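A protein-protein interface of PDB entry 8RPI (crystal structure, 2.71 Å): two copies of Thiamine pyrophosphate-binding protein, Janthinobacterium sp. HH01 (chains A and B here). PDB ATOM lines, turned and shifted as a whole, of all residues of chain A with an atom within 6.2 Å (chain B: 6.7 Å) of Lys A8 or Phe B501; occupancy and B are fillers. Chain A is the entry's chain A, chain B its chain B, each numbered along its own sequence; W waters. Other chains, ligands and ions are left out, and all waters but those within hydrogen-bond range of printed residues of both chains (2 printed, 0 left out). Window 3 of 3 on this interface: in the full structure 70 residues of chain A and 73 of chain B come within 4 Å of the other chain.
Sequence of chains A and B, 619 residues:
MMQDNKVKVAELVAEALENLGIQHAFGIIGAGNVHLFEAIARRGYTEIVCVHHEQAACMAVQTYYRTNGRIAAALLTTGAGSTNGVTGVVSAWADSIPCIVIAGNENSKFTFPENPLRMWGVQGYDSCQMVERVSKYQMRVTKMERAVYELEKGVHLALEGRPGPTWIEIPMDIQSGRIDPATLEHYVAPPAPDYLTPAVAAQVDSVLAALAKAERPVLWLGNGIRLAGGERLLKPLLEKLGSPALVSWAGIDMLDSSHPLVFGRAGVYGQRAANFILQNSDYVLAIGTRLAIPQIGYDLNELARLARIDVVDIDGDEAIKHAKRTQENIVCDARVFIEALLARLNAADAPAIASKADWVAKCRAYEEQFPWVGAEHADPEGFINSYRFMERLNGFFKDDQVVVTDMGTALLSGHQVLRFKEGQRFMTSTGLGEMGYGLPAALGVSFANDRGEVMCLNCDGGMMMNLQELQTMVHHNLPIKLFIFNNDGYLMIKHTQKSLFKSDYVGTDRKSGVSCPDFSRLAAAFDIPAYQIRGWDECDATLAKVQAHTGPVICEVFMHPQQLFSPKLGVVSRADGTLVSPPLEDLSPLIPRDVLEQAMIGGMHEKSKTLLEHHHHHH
Lys A8 touches one residue of chain B.
Of the printed residues of chain B, Glu A38 touches Phe B501 (3.3 Å) and Ser B503 (3.2 Å).
Of the printed residues of chain A, Gln B497 touches Val A34 (3.8 Å).
Ser B499 touches none of the printed residues of chain A.
Lys B502 touches none of the printed residues of chain A.
The nearest residue of chain B that does not touch Lys A8 is Leu B500 (6.3 Å).
Among the printed residues, pairs that only touch across the chains: Lys A8 with Phe B501 (3.3 Å), Glu A38 with Phe B501 (3.3 Å), His A35 with Phe B501 (3.6 Å), Val A34 with Gln B497 (3.8 Å), Val A34 with Phe B501 (3.8 Å), Val A34 with Leu B500 (3.8 Å) and His A35 with Leu B500 (3.9 Å).
The side-chain hydroxyl of Ser B503 lies within hydrogen-bond range of the side-chain carboxylate of Glu A38, at 3.2 Å.
Water W2 lies within hydrogen-bond range of the backbone carbonyl oxygen (O) of Asp B504 (2.4 Å), the side-chain carboxylate (OE2) of Glu A38 (2.7 Å) and the side-chain hydroxyl (OG) of Ser B503 (3.2 Å).
Water W1 lies within hydrogen-bond range of the side-chain amide nitrogen (NE2) of Gln B497 (2.8 Å), the side-chain carboxylate (OE1) of Glu A38 (2.8 Å) and the backbone carbonyl oxygen (O) of Val A34 (3.2 Å).
The side-chain hydroxyl (OG) of Ser B503 lies close to the backbone carbonyl oxygen (O) of Phe B501, at 3.5 Å.
The side-chain amino group of Lys B498 sits at hydrogen-bond distance from the backbone carbonyl oxygen of Ser B503 (2.5 Å).
No position is printed for both chains.
Of the 8 pairs that touch across the chains among the printed residues, none has its exchanged pair printed and touching as well.
Hydrophobic or aromatic side chains of chain B that line the printed part of chain A: Leu B500 and Phe B501.
Among the printed residues, no Asp or Glu carboxylate lies within 4 Å of a Lys or Arg side-chain nitrogen of the other chain.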
ATOM      1  N   LYS A   6       5.273   3.602  -6.222  1.00  0.00           N
ATOM      2  CA  LYS A   6       4.381   3.419  -7.355  1.00  0.00           C
ATOM      3  C   LYS A   6       2.922   3.543  -6.933  1.00  0.00           C
ATOM      4  O   LYS A   6       2.556   3.278  -5.784  1.00  0.00           O
ATOM      5  CB  LYS A   6       4.621   2.059  -8.006  1.00  0.00           C
ATOM      6  CG  LYS A   6       6.002   1.913  -8.616  1.00  0.00           C
ATOM      7  CD  LYS A   6       6.145   0.576  -9.324  1.00  0.00           C
ATOM      8  CE  LYS A   6       7.544   0.389  -9.897  1.00  0.00           C
ATOM      9  NZ  LYS A   6       7.676  -0.895 -10.639  1.00  0.00           N
ATOM     10  N   VAL A   7       2.086   3.948  -7.887  1.00  0.00           N
ATOM     11  CA  VAL A   7       0.659   4.140  -7.668  1.00  0.00           C
ATOM     12  C   VAL A   7      -0.107   3.427  -8.772  1.00  0.00           C
ATOM     13  O   VAL A   7       0.314   3.422  -9.934  1.00  0.00           O
ATOM     14  CB  VAL A   7       0.286   5.637  -7.630  1.00  0.00           C
ATOM     15  CG1 VAL A   7      -1.203   5.811  -7.358  1.00  0.00           C
ATOM     16  CG2 VAL A   7       1.119   6.361  -6.585  1.00  0.00           C
ATOM     17  N   LYS A   8      -1.240   2.834  -8.406  1.00  0.00           N
ATOM     18  CA  LYS A   8      -2.069   2.129  -9.374  1.00  0.00           C
ATOM     19  C   LYS A   8      -2.607   3.089 -10.430  1.00  0.00           C
ATOM     20  O   LYS A   8      -3.096   4.178 -10.113  1.00  0.00           O
ATOM     21  CB  LYS A   8      -3.219   1.433  -8.652  1.00  0.00           C
ATOM     22  CG  LYS A   8      -4.040   0.489  -9.508  1.00  0.00           C
ATOM     23  CD  LYS A   8      -5.116  -0.163  -8.657  1.00  0.00           C
ATOM     24  CE  LYS A   8      -6.043  -1.043  -9.465  1.00  0.00           C
ATOM     25  NZ  LYS A   8      -6.944  -1.802  -8.562  1.00  0.00           N
ATOM     26  N   VAL A   9      -2.522   2.671 -11.695  1.00  0.00           N
ATOM     27  CA  VAL A   9      -2.930   3.534 -12.801  1.00  0.00           C
ATOM     28  C   VAL A   9      -4.382   3.962 -12.639  1.00  0.00           C
ATOM     29  O   VAL A   9      -4.728   5.132 -12.848  1.00  0.00           O
ATOM     30  CB  VAL A   9      -2.695   2.818 -14.145  1.00  0.00           C
ATOM     31  CG1 VAL A   9      -3.337   3.587 -15.293  1.00  0.00           C
ATOM     32  CG2 VAL A   9      -1.207   2.647 -14.396  1.00  0.00           C
ATOM     33  N   ALA A  10      -5.256   3.025 -12.266  1.00  0.00           N
ATOM     34  CA  ALA A  10      -6.659   3.366 -12.061  1.00  0.00           C
ATOM     35  C   ALA A  10      -6.813   4.524 -11.079  1.00  0.00           C
ATOM     36  O   ALA A  10      -7.711   5.360 -11.234  1.00  0.00           O
ATOM     37  CB  ALA A  10      -7.423   2.132 -11.575  1.00  0.00           C
ATOM     38  N   GLU A  11      -5.942   4.602 -10.072  1.00  0.00           N
ATOM     39  CA  GLU A  11      -6.021   5.692  -9.107  1.00  0.00           C
ATOM     40  C   GLU A  11      -5.504   6.999  -9.691  1.00  0.00           C
ATOM     41  O   GLU A  11      -6.016   8.071  -9.348  1.00  0.00           O
ATOM     42  CB  GLU A  11      -5.250   5.319  -7.839  1.00  0.00           C
ATOM     43  CG  GLU A  11      -5.812   4.090  -7.129  1.00  0.00           C
ATOM     44  CD  GLU A  11      -5.022   3.701  -5.894  1.00  0.00           C
ATOM     45  OE1 GLU A  11      -4.053   4.414  -5.558  1.00  0.00           O
ATOM     46  OE2 GLU A  11      -5.373   2.681  -5.260  1.00  0.00           O
ATOM     47  N   LEU A  12      -4.501   6.938 -10.571  1.00  0.00           N
ATOM     48  CA  LEU A  12      -4.074   8.146 -11.269  1.00  0.00           C
ATOM     49  C   LEU A  12      -5.149   8.631 -12.231  1.00  0.00           C
ATOM     50  O   LEU A  12      -5.291   9.840 -12.447  1.00  0.00           O
ATOM     51  CB  LEU A  12      -2.767   7.887 -12.018  1.00  0.00           C
ATOM     52  CG  LEU A  12      -1.579   7.458 -11.153  1.00  0.00           C
ATOM     53  CD1 LEU A  12      -0.369   7.144 -12.025  1.00  0.00           C
ATOM     54  CD2 LEU A  12      -1.242   8.527 -10.111  1.00  0.00           C
ATOM     55  N   VAL A  13      -5.907   7.702 -12.814  1.00  0.00           N
ATOM     56  CA  VAL A  13      -7.027   8.075 -13.672  1.00  0.00           C
ATOM     57  C   VAL A  13      -8.090   8.802 -12.858  1.00  0.00           C
ATOM     58  O   VAL A  13      -8.605   9.848 -13.269  1.00  0.00           O
ATOM     59  CB  VAL A  13      -7.595   6.825 -14.368  1.00  0.00           C
ATOM     60  CG1 VAL A  13      -8.904   7.131 -15.054  1.00  0.00           C
ATOM     61  CG2 VAL A  13      -6.600   6.295 -15.384  1.00  0.00           C
ATOM     62  N   VAL A  34     -13.700  -2.742 -13.678  1.00  0.00           N
ATOM     63  CA  VAL A  34     -13.895  -2.879 -12.239  1.00  0.00           C
ATOM     64  C   VAL A  34     -12.810  -2.134 -11.467  1.00  0.00           C
ATOM     65  O   VAL A  34     -13.052  -1.649 -10.355  1.00  0.00           O
ATOM     66  CB  VAL A  34     -13.948  -4.372 -11.856  1.00  0.00           C
ATOM     67  CG1 VAL A  34     -12.601  -5.057 -12.110  1.00  0.00           C
ATOM     68  CG2 VAL A  34     -14.378  -4.531 -10.414  1.00  0.00           C
ATOM     69  N   HIS A  35     -11.632  -2.020 -12.019  1.00  0.00           N
ATOM     70  CA  HIS A  35     -10.579  -1.273 -11.398  1.00  0.00           C
ATOM     71  C   HIS A  35     -10.842   0.194 -11.397  1.00  0.00           C
ATOM     72  O   HIS A  35     -10.420   0.866 -10.525  1.00  0.00           O
ATOM     73  CB  HIS A  35      -9.260  -1.555 -12.056  1.00  0.00           C
ATOM     74  CG  HIS A  35      -8.753  -2.918 -11.793  1.00  0.00           C
ATOM     75  ND1 HIS A  35      -8.812  -3.914 -12.723  1.00  0.00           N
ATOM     76  CD2 HIS A  35      -8.212  -3.463 -10.697  1.00  0.00           C
ATOM     77  CE1 HIS A  35      -8.321  -5.015 -12.215  1.00  0.00           C
ATOM     78  NE2 HIS A  35      -7.941  -4.763 -10.989  1.00  0.00           N
ATOM     79  N   LEU A  36     -11.449   0.705 -12.442  1.00  0.00           N
ATOM     80  CA  LEU A  36     -11.752   2.127 -12.519  1.00  0.00           C
ATOM     81  C   LEU A  36     -12.920   2.484 -11.609  1.00  0.00           C
ATOM     82  O   LEU A  36     -12.901   3.534 -10.959  1.00  0.00           O
ATOM     83  CB  LEU A  36     -12.039   2.524 -13.970  1.00  0.00           C
ATOM     84  CG  LEU A  36     -10.844   2.400 -14.926  1.00  0.00           C
ATOM     85  CD1 LEU A  36     -11.258   2.607 -16.378  1.00  0.00           C
ATOM     86  CD2 LEU A  36      -9.752   3.389 -14.566  1.00  0.00           C
ATOM     87  N   GLU A  38     -13.598   1.053  -8.769  1.00  0.00           N
ATOM     88  CA  GLU A  38     -13.069   1.050  -7.408  1.00  0.00           C
ATOM     89  C   GLU A  38     -12.261   2.312  -7.127  1.00  0.00           C
ATOM     90  O   GLU A  38     -12.466   2.979  -6.108  1.00  0.00           O
ATOM     91  CB  GLU A  38     -12.211  -0.198  -7.186  1.00  0.00           C
ATOM     92  CG  GLU A  38     -11.845  -0.454  -5.731  1.00  0.00           C
ATOM     93  CD  GLU A  38     -13.008  -0.973  -4.907  1.00  0.00           C
ATOM     94  OE1 GLU A  38     -13.890  -1.664  -5.468  1.00  0.00           O
ATOM     95  OE2 GLU A  38     -13.031  -0.688  -3.691  1.00  0.00           O
ATOM     96  N   ALA A  39     -11.326   2.650  -8.020  1.00  0.00           N
ATOM     97  CA  ALA A  39     -10.474   3.813  -7.788  1.00  0.00           C
ATOM     98  C   ALA A  39     -11.290   5.099  -7.740  1.00  0.00           C
ATOM     99  O   ALA A  39     -11.001   5.994  -6.938  1.00  0.00           O
ATOM    100  CB  ALA A  39      -9.400   3.905  -8.871  1.00  0.00           C
ATOM    101  N   GLN A 175      -5.192  -0.713 -16.506  1.00  0.00           N
ATOM    102  CA  GLN A 175      -5.848  -0.114 -15.349  1.00  0.00           C
ATOM    103  C   GLN A 175      -5.202  -0.572 -14.049  1.00  0.00           C
ATOM    104  O   GLN A 175      -5.040   0.223 -13.116  1.00  0.00           O
ATOM    105  CB  GLN A 175      -7.334  -0.463 -15.342  1.00  0.00           C
ATOM    106  CG  GLN A 175      -8.075  -0.033 -16.584  1.00  0.00           C
ATOM    107  CD  GLN A 175      -9.469  -0.613 -16.649  1.00  0.00           C
ATOM    108  OE1 GLN A 175     -10.027  -1.045 -15.638  1.00  0.00           O
ATOM    109  NE2 GLN A 175     -10.038  -0.640 -17.847  1.00  0.00           N
ATOM    110  N   SER A 176      -4.821  -1.847 -13.973  1.00  0.00           N
ATOM    111  CA  SER A 176      -4.345  -2.444 -12.733  1.00  0.00           C
ATOM    112  C   SER A 176      -2.839  -2.321 -12.538  1.00  0.00           C
ATOM    113  O   SER A 176      -2.349  -2.608 -11.441  1.00  0.00           O
ATOM    114  CB  SER A 176      -4.739  -3.922 -12.687  1.00  0.00           C
ATOM    115  OG  SER A 176      -4.213  -4.609 -13.810  1.00  0.00           O
ATOM    116  N   GLY A 177      -2.099  -1.909 -13.560  1.00  0.00           N
ATOM    117  CA  GLY A 177      -0.666  -1.737 -13.425  1.00  0.00           C
ATOM    118  C   GLY A 177      -0.300  -0.682 -12.397  1.00  0.00           C
ATOM    119  O   GLY A 177      -1.138   0.026 -11.838  1.00  0.00           O
ATOM    120  N   ARG A 178       1.006  -0.583 -12.150  1.00  0.00           N
ATOM    121  CA  ARG A 178       1.555   0.328 -11.154  1.00  0.00           C
ATOM    122  C   ARG A 178       2.774   1.025 -11.738  1.00  0.00           C
ATOM    123  O   ARG A 178       3.648   0.368 -12.308  1.00  0.00           O
ATOM    124  CB  ARG A 178       1.945  -0.421  -9.872  1.00  0.00           C
ATOM    125  CG  ARG A 178       0.811  -1.205  -9.223  1.00  0.00           C
ATOM    126  CD  ARG A 178       1.289  -1.957  -7.980  1.00  0.00           C
ATOM    127  NE  ARG A 178       1.858  -1.063  -6.977  1.00  0.00           N
ATOM    128  CZ  ARG A 178       1.152  -0.409  -6.065  1.00  0.00           C
ATOM    129  NH1 ARG A 178      -0.166  -0.518  -6.000  1.00  0.00           N
ATOM    130  NH2 ARG A 178       1.783   0.377  -5.197  1.00  0.00           N
ATOM    131  N   ILE A 179       2.834   2.350 -11.588  1.00  0.00           N
ATOM    132  CA  ILE A 179       3.950   3.153 -12.074  1.00  0.00           C
ATOM    133  C   ILE A 179       4.275   4.233 -11.049  1.00  0.00           C
ATOM    134  O   ILE A 179       3.498   4.515 -10.135  1.00  0.00           O
ATOM    135  CB  ILE A 179       3.654   3.800 -13.444  1.00  0.00           C
ATOM    136  CG1 ILE A 179       2.383   4.652 -13.364  1.00  0.00           C
ATOM    137  CG2 ILE A 179       3.531   2.729 -14.501  1.00  0.00           C
ATOM    138  CD1 ILE A 179       2.050   5.399 -14.643  1.00  0.00           C
ATOM    139  N   THR B 496     -16.043 -10.799  -8.173  1.00  0.00           N
ATOM    140  CA  THR B 496     -14.862 -10.284  -8.856  1.00  0.00           C
ATOM    141  C   THR B 496     -14.189  -9.185  -8.038  1.00  0.00           C
ATOM    142  O   THR B 496     -12.987  -9.254  -7.757  1.00  0.00           O
ATOM    143  CB  THR B 496     -15.249  -9.775 -10.245  1.00  0.00           C
ATOM    144  OG1 THR B 496     -15.812 -10.850 -11.004  1.00  0.00           O
ATOM    145  CG2 THR B 496     -14.039  -9.229 -10.980  1.00  0.00           C
ATOM    146  N   GLN B 497     -14.945  -8.159  -7.643  1.00  0.00           N
ATOM    147  CA  GLN B 497     -14.322  -7.053  -6.922  1.00  0.00           C
ATOM    148  C   GLN B 497     -13.953  -7.448  -5.496  1.00  0.00           C
ATOM    149  O   GLN B 497     -13.007  -6.890  -4.928  1.00  0.00           O
ATOM    150  CB  GLN B 497     -15.240  -5.825  -6.927  1.00  0.00           C
ATOM    151  CG  GLN B 497     -16.608  -6.044  -6.304  1.00  0.00           C
ATOM    152  CD  GLN B 497     -17.545  -4.846  -6.444  1.00  0.00           C
ATOM    153  OE1 GLN B 497     -18.617  -4.827  -5.842  1.00  0.00           O
ATOM    154  NE2 GLN B 497     -17.151  -3.849  -7.240  1.00  0.00           N
ATOM    155  N   LYS B 498     -14.652  -8.397  -4.906  1.00  0.00           N
ATOM    156  CA  LYS B 498     -14.298  -8.886  -3.586  1.00  0.00           C
ATOM    157  C   LYS B 498     -12.971  -9.625  -3.621  1.00  0.00           C
ATOM    158  O   LYS B 498     -12.161  -9.456  -2.768  1.00  0.00           O
ATOM    159  CB  LYS B 498     -15.381  -9.791  -3.063  1.00  0.00           C
ATOM    160  CG  LYS B 498     -15.590  -9.715  -1.579  1.00  0.00           C
ATOM    161  CD  LYS B 498     -16.096  -8.349  -1.159  1.00  0.00           C
ATOM    162  CE  LYS B 498     -16.619  -8.282   0.269  1.00  0.00           C
ATOM    163  NZ  LYS B 498     -17.022  -6.902   0.615  1.00  0.00           N
ATOM    164  N   SER B 499     -12.737 -10.453  -4.616  1.00  0.00           N
ATOM    165  CA  SER B 499     -11.458 -11.147  -4.730  1.00  0.00           C
ATOM    166  C   SER B 499     -10.317 -10.183  -5.029  1.00  0.00           C
ATOM    167  O   SER B 499      -9.165 -10.465  -4.684  1.00  0.00           O
ATOM    168  CB  SER B 499     -11.517 -12.211  -5.830  1.00  0.00           C
ATOM    169  OG  SER B 499     -12.636 -13.065  -5.684  1.00  0.00           O
ATOM    170  N   LEU B 500     -10.608  -9.056  -5.676  1.00  0.00           N
ATOM    171  CA  LEU B 500      -9.576  -8.105  -6.072  1.00  0.00           C
ATOM    172  C   LEU B 500      -9.265  -7.079  -4.989  1.00  0.00           C
ATOM    173  O   LEU B 500      -8.099  -6.718  -4.795  1.00  0.00           O
ATOM    174  CB  LEU B 500     -10.005  -7.368  -7.346  1.00  0.00           C
ATOM    175  CG  LEU B 500      -9.987  -8.169  -8.648  1.00  0.00           C
ATOM    176  CD1 LEU B 500     -10.607  -7.359  -9.775  1.00  0.00           C
ATOM    177  CD2 LEU B 500      -8.565  -8.575  -9.001  1.00  0.00           C
ATOM    178  N   PHE B 501     -10.287  -6.588  -4.290  1.00  0.00           N
ATOM    179  CA  PHE B 501     -10.118  -5.467  -3.379  1.00  0.00           C
ATOM    180  C   PHE B 501     -10.470  -5.776  -1.935  1.00  0.00           C
ATOM    181  O   PHE B 501     -10.078  -5.006  -1.052  1.00  0.00           O
ATOM    182  CB  PHE B 501     -10.966  -4.273  -3.845  1.00  0.00           C
ATOM    183  CG  PHE B 501     -10.842  -3.985  -5.309  1.00  0.00           C
ATOM    184  CD1 PHE B 501      -9.659  -3.496  -5.831  1.00  0.00           C
ATOM    185  CD2 PHE B 501     -11.905  -4.208  -6.163  1.00  0.00           C
ATOM    186  CE1 PHE B 501      -9.538  -3.234  -7.178  1.00  0.00           C
ATOM    187  CE2 PHE B 501     -11.794  -3.946  -7.511  1.00  0.00           C
ATOM    188  CZ  PHE B 501     -10.608  -3.458  -8.020  1.00  0.00           C
ATOM    189  N   LYS B 502     -11.191  -6.861  -1.667  1.00  0.00           N
ATOM    190  CA  LYS B 502     -11.563  -7.231  -0.306  1.00  0.00           C
ATOM    191  C   LYS B 502     -12.030  -6.007   0.474  1.00  0.00           C
ATOM    192  O   LYS B 502     -11.534  -5.693   1.558  1.00  0.00           O
ATOM    193  CB  LYS B 502     -10.402  -7.926   0.400  1.00  0.00           C
ATOM    194  CG  LYS B 502     -10.040  -9.271  -0.208  1.00  0.00           C
ATOM    195  CD  LYS B 502      -8.702  -9.781   0.308  1.00  0.00           C
ATOM    196  CE  LYS B 502      -8.482 -11.255  -0.016  1.00  0.00           C
ATOM    197  NZ  LYS B 502      -8.608 -11.558  -1.470  1.00  0.00           N
ATOM    198  N   SER B 503     -12.988  -5.294  -0.107  1.00  0.00           N
ATOM    199  CA  SER B 503     -13.570  -4.124   0.535  1.00  0.00           C
ATOM    200  C   SER B 503     -15.054  -4.084   0.185  1.00  0.00           C
ATOM    201  O   SER B 503     -15.625  -5.062  -0.308  1.00  0.00           O
ATOM    202  CB  SER B 503     -12.811  -2.853   0.127  1.00  0.00           C
ATOM    203  OG  SER B 503     -12.717  -2.730  -1.278  1.00  0.00           O
ATOM    204  N   ASP B 504     -15.687  -2.950   0.466  1.00  0.00           N
ATOM    205  CA  ASP B 504     -17.120  -2.821   0.261  1.00  0.00           C
ATOM    206  C   ASP B 504     -17.468  -2.839  -1.221  1.00  0.00           C
ATOM    207  O   ASP B 504     -16.681  -2.426  -2.078  1.00  0.00           O
ATOM    208  CB  ASP B 504     -17.636  -1.528   0.889  1.00  0.00           C
ATOM    209  CG  ASP B 504     -17.588  -1.552   2.405  1.00  0.00           C
ATOM    210  OD1 ASP B 504     -17.226  -2.602   2.978  1.00  0.00           O
ATOM    211  OD2 ASP B 504     -17.911  -0.516   3.026  1.00  0.00           O
HETATM  212  O   HOH W   1     -15.061  -2.199  -7.977  1.00  0.00           O
HETATM  213  O   HOH W   2     -15.038  -0.621  -1.927  1.00  0.00           O
